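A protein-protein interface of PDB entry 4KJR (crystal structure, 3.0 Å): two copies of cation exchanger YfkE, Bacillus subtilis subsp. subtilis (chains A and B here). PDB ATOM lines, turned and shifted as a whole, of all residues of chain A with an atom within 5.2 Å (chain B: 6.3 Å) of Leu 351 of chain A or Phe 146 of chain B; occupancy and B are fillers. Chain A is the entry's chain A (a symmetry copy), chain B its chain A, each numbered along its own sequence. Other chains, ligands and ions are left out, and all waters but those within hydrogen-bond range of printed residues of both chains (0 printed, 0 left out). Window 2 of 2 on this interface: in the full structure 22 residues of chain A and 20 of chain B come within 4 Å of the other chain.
No position is printed for both chains.
Of the 11 pairs that touch across the chains among the printed residues, none has its exchanged pair printed and touching as well.
Hydrophobic or aromatic side chains of chain A that line the printed part of chain B: Trp 237, Pro 308, Phe 348, Leu 350 and Leu 351.
Leu 351 of chain A touches one residue of chain B.
Printed residues of chain B within 4 Å of Pro 308 of chain A: Val 145 (3.7 Å) and Phe 146 (3.4 Å).
Of the printed residues of chain A, Ser 154 of chain B touches Leu 350 (3.5 Å).
Of the printed residues of chain A, Val 145 of chain B touches Pro 308.
Printed residues of chain B within 4 Å of Gly 347 of chain A: Phe 146 (3.4 Å) and Leu 158 (3.7 Å).
The nearest residue of chain B that does not touch Leu 351 of chain A is Gly 149 of chain B (4.2 Å).
The nearest printed residue of chain B that does not touch Phe 348 of chain A is Leu 158 of chain B (6.1 Å).
OG of Ser 238 of chain A is in hydrogen-bond range of O of Leu 351 of chain A (3.1 Å).
CH2 of Trp 237 of chain A touches O of Met 150 of chain B, at 3.2 Å.
CG1 of Val 145 of chain B touches N of Pro 308 of chain A, 3.7 Å away.
O of Pro 308 of chain A touches CE2 of Phe 146 of chain B, at 3.4 Å.
CE1 of Phe 146 of chain B touches O of Met 344 of chain A (3.9 Å).
Phe 146 of chain B touches Gly 347 of chain A.
Phe 348 of chain A touches Phe 146 of chain B.
Leu 350 of chain A touches Met 150 of chain B.
Ser 154 of chain B touches Leu 350 of chain A (O to CD2, 3.5 Å).
N of Leu 158 of chain B touches CD2 of Leu 350 of chain A, 3.8 Å away.
Leu 351 of chain A touches Phe 146 of chain B.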
ATOM      1  N   TRP A 237     -21.020 -33.493  -0.271  1.00  0.00           N
ATOM      2  CA  TRP A 237     -21.553 -33.966   1.001  1.00  0.00           C
ATOM      3  C   TRP A 237     -22.418 -32.865   1.549  1.00  0.00           C
ATOM      4  O   TRP A 237     -22.439 -31.773   0.980  1.00  0.00           O
ATOM      5  CB  TRP A 237     -20.403 -34.309   1.962  1.00  0.00           C
ATOM      6  CG  TRP A 237     -19.189 -33.404   1.866  1.00  0.00           C
ATOM      7  CD1 TRP A 237     -18.830 -32.562   0.813  1.00  0.00           C
ATOM      8  CD2 TRP A 237     -18.104 -33.254   2.850  1.00  0.00           C
ATOM      9  NE1 TRP A 237     -17.651 -31.914   1.075  1.00  0.00           N
ATOM     10  CE2 TRP A 237     -17.160 -32.284   2.274  1.00  0.00           C
ATOM     11  CE3 TRP A 237     -17.828 -33.804   4.095  1.00  0.00           C
ATOM     12  CZ2 TRP A 237     -16.005 -31.896   2.941  1.00  0.00           C
ATOM     13  CZ3 TRP A 237     -16.665 -33.397   4.763  1.00  0.00           C
ATOM     14  CH2 TRP A 237     -15.777 -32.469   4.197  1.00  0.00           C
ATOM     15  N   SER A 238     -23.163 -33.115   2.627  1.00  0.00           N
ATOM     16  CA  SER A 238     -23.244 -34.419   3.279  1.00  0.00           C
ATOM     17  C   SER A 238     -24.670 -34.841   3.565  1.00  0.00           C
ATOM     18  O   SER A 238     -25.623 -34.104   3.287  1.00  0.00           O
ATOM     19  CB  SER A 238     -22.441 -34.409   4.581  1.00  0.00           C
ATOM     20  OG  SER A 238     -21.058 -34.233   4.327  1.00  0.00           O
ATOM     21  N   PRO A 308     -22.258 -28.121  15.803  1.00  0.00           N
ATOM     22  CA  PRO A 308     -22.493 -27.189  14.699  1.00  0.00           C
ATOM     23  C   PRO A 308     -23.969 -26.857  14.474  1.00  0.00           C
ATOM     24  O   PRO A 308     -24.293 -25.715  14.120  1.00  0.00           O
ATOM     25  CB  PRO A 308     -21.928 -27.934  13.482  1.00  0.00           C
ATOM     26  CG  PRO A 308     -21.778 -29.361  13.913  1.00  0.00           C
ATOM     27  CD  PRO A 308     -21.458 -29.279  15.366  1.00  0.00           C
ATOM     28  N   ALA A 312     -25.543 -23.025  15.753  1.00  0.00           N
ATOM     29  CA  ALA A 312     -26.283 -22.360  14.688  1.00  0.00           C
ATOM     30  C   ALA A 312     -27.665 -21.894  15.129  1.00  0.00           C
ATOM     31  O   ALA A 312     -28.073 -20.772  14.809  1.00  0.00           O
ATOM     32  CB  ALA A 312     -26.407 -23.288  13.497  1.00  0.00           C
ATOM     33  N   MET A 344     -24.112 -20.031   7.193  1.00  0.00           N
ATOM     34  CA  MET A 344     -24.363 -21.295   7.892  1.00  0.00           C
ATOM     35  C   MET A 344     -24.585 -22.428   6.930  1.00  0.00           C
ATOM     36  O   MET A 344     -24.093 -23.538   7.156  1.00  0.00           O
ATOM     37  CB  MET A 344     -25.540 -21.134   8.835  1.00  0.00           C
ATOM     38  CG  MET A 344     -25.055 -20.349  10.043  1.00  0.00           C
ATOM     39  SD  MET A 344     -26.466 -20.367  11.410  1.00  0.00           S
ATOM     40  CE  MET A 344     -26.390 -18.454  11.887  1.00  0.00           C
ATOM     41  N   GLY A 347     -21.203 -23.501   5.543  1.00  0.00           N
ATOM     42  CA  GLY A 347     -20.560 -24.259   6.612  1.00  0.00           C
ATOM     43  C   GLY A 347     -21.117 -25.670   6.715  1.00  0.00           C
ATOM     44  O   GLY A 347     -20.366 -26.640   6.797  1.00  0.00           O
ATOM     45  N   PHE A 348     -22.443 -25.783   6.701  1.00  0.00           N
ATOM     46  CA  PHE A 348     -23.107 -27.081   6.783  1.00  0.00           C
ATOM     47  C   PHE A 348     -22.807 -27.970   5.584  1.00  0.00           C
ATOM     48  O   PHE A 348     -22.847 -29.189   5.697  1.00  0.00           O
ATOM     49  CB  PHE A 348     -24.622 -26.920   6.962  1.00  0.00           C
ATOM     50  CG  PHE A 348     -25.048 -26.790   8.396  1.00  0.00           C
ATOM     51  CD1 PHE A 348     -24.924 -27.864   9.271  1.00  0.00           C
ATOM     52  CD2 PHE A 348     -25.562 -25.600   8.875  1.00  0.00           C
ATOM     53  CE1 PHE A 348     -25.301 -27.750  10.598  1.00  0.00           C
ATOM     54  CE2 PHE A 348     -25.950 -25.479  10.200  1.00  0.00           C
ATOM     55  CZ  PHE A 348     -25.816 -26.555  11.063  1.00  0.00           C
ATOM     56  N   PHE A 349     -22.505 -27.352   4.443  1.00  0.00           N
ATOM     57  CA  PHE A 349     -22.162 -28.088   3.224  1.00  0.00           C
ATOM     58  C   PHE A 349     -20.740 -28.631   3.305  1.00  0.00           C
ATOM     59  O   PHE A 349     -20.470 -29.771   2.912  1.00  0.00           O
ATOM     60  CB  PHE A 349     -22.343 -27.197   1.990  1.00  0.00           C
ATOM     61  CG  PHE A 349     -21.595 -27.674   0.773  1.00  0.00           C
ATOM     62  CD1 PHE A 349     -21.947 -28.862   0.142  1.00  0.00           C
ATOM     63  CD2 PHE A 349     -20.555 -26.923   0.239  1.00  0.00           C
ATOM     64  CE1 PHE A 349     -21.261 -29.299  -0.982  1.00  0.00           C
ATOM     65  CE2 PHE A 349     -19.866 -27.353  -0.881  1.00  0.00           C
ATOM     66  CZ  PHE A 349     -20.221 -28.541  -1.495  1.00  0.00           C
ATOM     67  N   LEU A 350     -19.844 -27.805   3.841  1.00  0.00           N
ATOM     68  CA  LEU A 350     -18.440 -28.167   4.002  1.00  0.00           C
ATOM     69  C   LEU A 350     -18.227 -29.358   4.939  1.00  0.00           C
ATOM     70  O   LEU A 350     -17.327 -30.162   4.720  1.00  0.00           O
ATOM     71  CB  LEU A 350     -17.619 -26.944   4.422  1.00  0.00           C
ATOM     72  CG  LEU A 350     -16.910 -26.162   3.301  1.00  0.00           C
ATOM     73  CD1 LEU A 350     -17.656 -26.199   1.973  1.00  0.00           C
ATOM     74  CD2 LEU A 350     -16.611 -24.720   3.702  1.00  0.00           C
ATOM     75  N   LEU A 351     -19.063 -29.486   5.963  1.00  0.00           N
ATOM     76  CA  LEU A 351     -19.050 -30.677   6.813  1.00  0.00           C
ATOM     77  C   LEU A 351     -19.414 -31.943   6.046  1.00  0.00           C
ATOM     78  O   LEU A 351     -19.092 -33.052   6.476  1.00  0.00           O
ATOM     79  CB  LEU A 351     -19.989 -30.509   8.011  1.00  0.00           C
ATOM     80  CG  LEU A 351     -19.457 -29.688   9.185  1.00  0.00           C
ATOM     81  CD1 LEU A 351     -20.583 -29.372  10.157  1.00  0.00           C
ATOM     82  CD2 LEU A 351     -18.341 -30.440   9.884  1.00  0.00           C
ATOM     83  N   VAL B 141     -17.547 -17.294  15.950  1.00  0.00           N
ATOM     84  CA  VAL B 141     -18.128 -18.536  16.501  1.00  0.00           C
ATOM     85  C   VAL B 141     -18.357 -19.615  15.439  1.00  0.00           C
ATOM     86  O   VAL B 141     -17.886 -20.738  15.592  1.00  0.00           O
ATOM     87  CB  VAL B 141     -19.444 -18.277  17.265  1.00  0.00           C
ATOM     88  CG1 VAL B 141     -20.239 -19.553  17.436  1.00  0.00           C
ATOM     89  CG2 VAL B 141     -19.174 -17.666  18.619  1.00  0.00           C
ATOM     90  N   ILE B 142     -19.064 -19.271  14.367  1.00  0.00           N
ATOM     91  CA  ILE B 142     -19.361 -20.246  13.312  1.00  0.00           C
ATOM     92  C   ILE B 142     -18.086 -20.929  12.810  1.00  0.00           C
ATOM     93  O   ILE B 142     -18.004 -22.152  12.844  1.00  0.00           O
ATOM     94  CB  ILE B 142     -20.160 -19.661  12.121  1.00  0.00           C
ATOM     95  CG1 ILE B 142     -21.321 -18.765  12.578  1.00  0.00           C
ATOM     96  CG2 ILE B 142     -20.667 -20.771  11.221  1.00  0.00           C
ATOM     97  CD1 ILE B 142     -21.777 -18.948  14.015  1.00  0.00           C
ATOM     98  N   PRO B 143     -17.086 -20.149  12.357  1.00  0.00           N
ATOM     99  CA  PRO B 143     -15.814 -20.741  11.972  1.00  0.00           C
ATOM    100  C   PRO B 143     -15.252 -21.735  12.982  1.00  0.00           C
ATOM    101  O   PRO B 143     -14.876 -22.838  12.597  1.00  0.00           O
ATOM    102  CB  PRO B 143     -14.899 -19.533  11.868  1.00  0.00           C
ATOM    103  CG  PRO B 143     -15.791 -18.469  11.382  1.00  0.00           C
ATOM    104  CD  PRO B 143     -17.158 -18.738  11.943  1.00  0.00           C
ATOM    105  N   GLU B 144     -15.197 -21.342  14.254  1.00  0.00           N
ATOM    106  CA  GLU B 144     -14.646 -22.201  15.303  1.00  0.00           C
ATOM    107  C   GLU B 144     -15.342 -23.554  15.393  1.00  0.00           C
ATOM    108  O   GLU B 144     -14.680 -24.589  15.328  1.00  0.00           O
ATOM    109  CB  GLU B 144     -14.674 -21.511  16.666  1.00  0.00           C
ATOM    110  CG  GLU B 144     -13.306 -21.195  17.237  1.00  0.00           C
ATOM    111  CD  GLU B 144     -13.269 -21.267  18.763  1.00  0.00           C
ATOM    112  OE1 GLU B 144     -13.728 -22.274  19.347  1.00  0.00           O
ATOM    113  OE2 GLU B 144     -12.753 -20.325  19.393  1.00  0.00           O
ATOM    114  N   VAL B 145     -16.666 -23.551  15.527  1.00  0.00           N
ATOM    115  CA  VAL B 145     -17.398 -24.809  15.731  1.00  0.00           C
ATOM    116  C   VAL B 145     -17.345 -25.689  14.487  1.00  0.00           C
ATOM    117  O   VAL B 145     -16.929 -26.843  14.557  1.00  0.00           O
ATOM    118  CB  VAL B 145     -18.871 -24.613  16.163  1.00  0.00           C
ATOM    119  CG1 VAL B 145     -19.405 -25.914  16.744  1.00  0.00           C
ATOM    120  CG2 VAL B 145     -19.003 -23.494  17.188  1.00  0.00           C
ATOM    121  N   PHE B 146     -17.757 -25.118  13.358  1.00  0.00           N
ATOM    122  CA  PHE B 146     -17.786 -25.804  12.063  1.00  0.00           C
ATOM    123  C   PHE B 146     -16.430 -26.347  11.599  1.00  0.00           C
ATOM    124  O   PHE B 146     -16.376 -27.348  10.897  1.00  0.00           O
ATOM    125  CB  PHE B 146     -18.378 -24.875  11.001  1.00  0.00           C
ATOM    126  CG  PHE B 146     -19.880 -24.757  11.069  1.00  0.00           C
ATOM    127  CD1 PHE B 146     -20.669 -25.181  10.005  1.00  0.00           C
ATOM    128  CD2 PHE B 146     -20.510 -24.244  12.199  1.00  0.00           C
ATOM    129  CE1 PHE B 146     -22.047 -25.085  10.055  1.00  0.00           C
ATOM    130  CE2 PHE B 146     -21.893 -24.145  12.256  1.00  0.00           C
ATOM    131  CZ  PHE B 146     -22.661 -24.566  11.182  1.00  0.00           C
ATOM    132  N   SER B 147     -15.342 -25.701  12.007  1.00  0.00           N
ATOM    133  CA  SER B 147     -14.010 -26.067  11.532  1.00  0.00           C
ATOM    134  C   SER B 147     -13.353 -27.210  12.299  1.00  0.00           C
ATOM    135  O   SER B 147     -12.237 -27.619  11.960  1.00  0.00           O
ATOM    136  CB  SER B 147     -13.079 -24.845  11.493  1.00  0.00           C
ATOM    137  OG  SER B 147     -13.009 -24.170  12.740  1.00  0.00           O
ATOM    138  N   VAL B 148     -14.044 -27.724  13.319  1.00  0.00           N
ATOM    139  CA  VAL B 148     -13.480 -28.747  14.211  1.00  0.00           C
ATOM    140  C   VAL B 148     -12.748 -29.859  13.458  1.00  0.00           C
ATOM    141  O   VAL B 148     -11.549 -30.052  13.652  1.00  0.00           O
ATOM    142  CB  VAL B 148     -14.521 -29.306  15.219  1.00  0.00           C
ATOM    143  CG1 VAL B 148     -15.683 -29.997  14.508  1.00  0.00           C
ATOM    144  CG2 VAL B 148     -13.851 -30.245  16.212  1.00  0.00           C
ATOM    145  N   GLY B 149     -13.463 -30.568  12.589  1.00  0.00           N
ATOM    146  CA  GLY B 149     -12.861 -31.586  11.724  1.00  0.00           C
ATOM    147  C   GLY B 149     -13.455 -31.500  10.329  1.00  0.00           C
ATOM    148  O   GLY B 149     -14.499 -32.100  10.055  1.00  0.00           O
ATOM    149  N   MET B 150     -12.797 -30.754   9.446  1.00  0.00           N
ATOM    150  CA  MET B 150     -13.372 -30.456   8.132  1.00  0.00           C
ATOM    151  C   MET B 150     -12.658 -31.086   6.939  1.00  0.00           C
ATOM    152  O   MET B 150     -13.328 -31.699   6.100  1.00  0.00           O
ATOM    153  CB  MET B 150     -13.602 -28.948   7.982  1.00  0.00           C
ATOM    154  CG  MET B 150     -15.087 -28.669   7.776  1.00  0.00           C
ATOM    155  SD  MET B 150     -15.544 -26.754   7.567  1.00  0.00           S
ATOM    156  CE  MET B 150     -13.813 -25.908   7.907  1.00  0.00           C
ATOM    157  N   SER B 154     -11.221 -27.038   3.621  1.00  0.00           N
ATOM    158  CA  SER B 154     -12.550 -26.513   3.945  1.00  0.00           C
ATOM    159  C   SER B 154     -12.505 -25.294   4.865  1.00  0.00           C
ATOM    160  O   SER B 154     -13.275 -24.338   4.674  1.00  0.00           O
ATOM    161  CB  SER B 154     -13.424 -27.600   4.561  1.00  0.00           C
ATOM    162  OG  SER B 154     -13.717 -28.603   3.606  1.00  0.00           O
ATOM    163  N   LEU B 158     -14.415 -21.665   4.057  1.00  0.00           N
ATOM    164  CA  LEU B 158     -15.442 -21.078   4.893  1.00  0.00           C
ATOM    165  C   LEU B 158     -15.032 -19.665   5.280  1.00  0.00           C
ATOM    166  O   LEU B 158     -15.807 -18.730   5.128  1.00  0.00           O
ATOM    167  CB  LEU B 158     -15.703 -21.928   6.137  1.00  0.00           C
ATOM    168  CG  LEU B 158     -16.934 -21.520   6.949  1.00  0.00           C
ATOM    169  CD1 LEU B 158     -18.174 -21.422   6.070  1.00  0.00           C
ATOM    170  CD2 LEU B 158     -17.157 -22.480   8.103  1.00  0.00           C
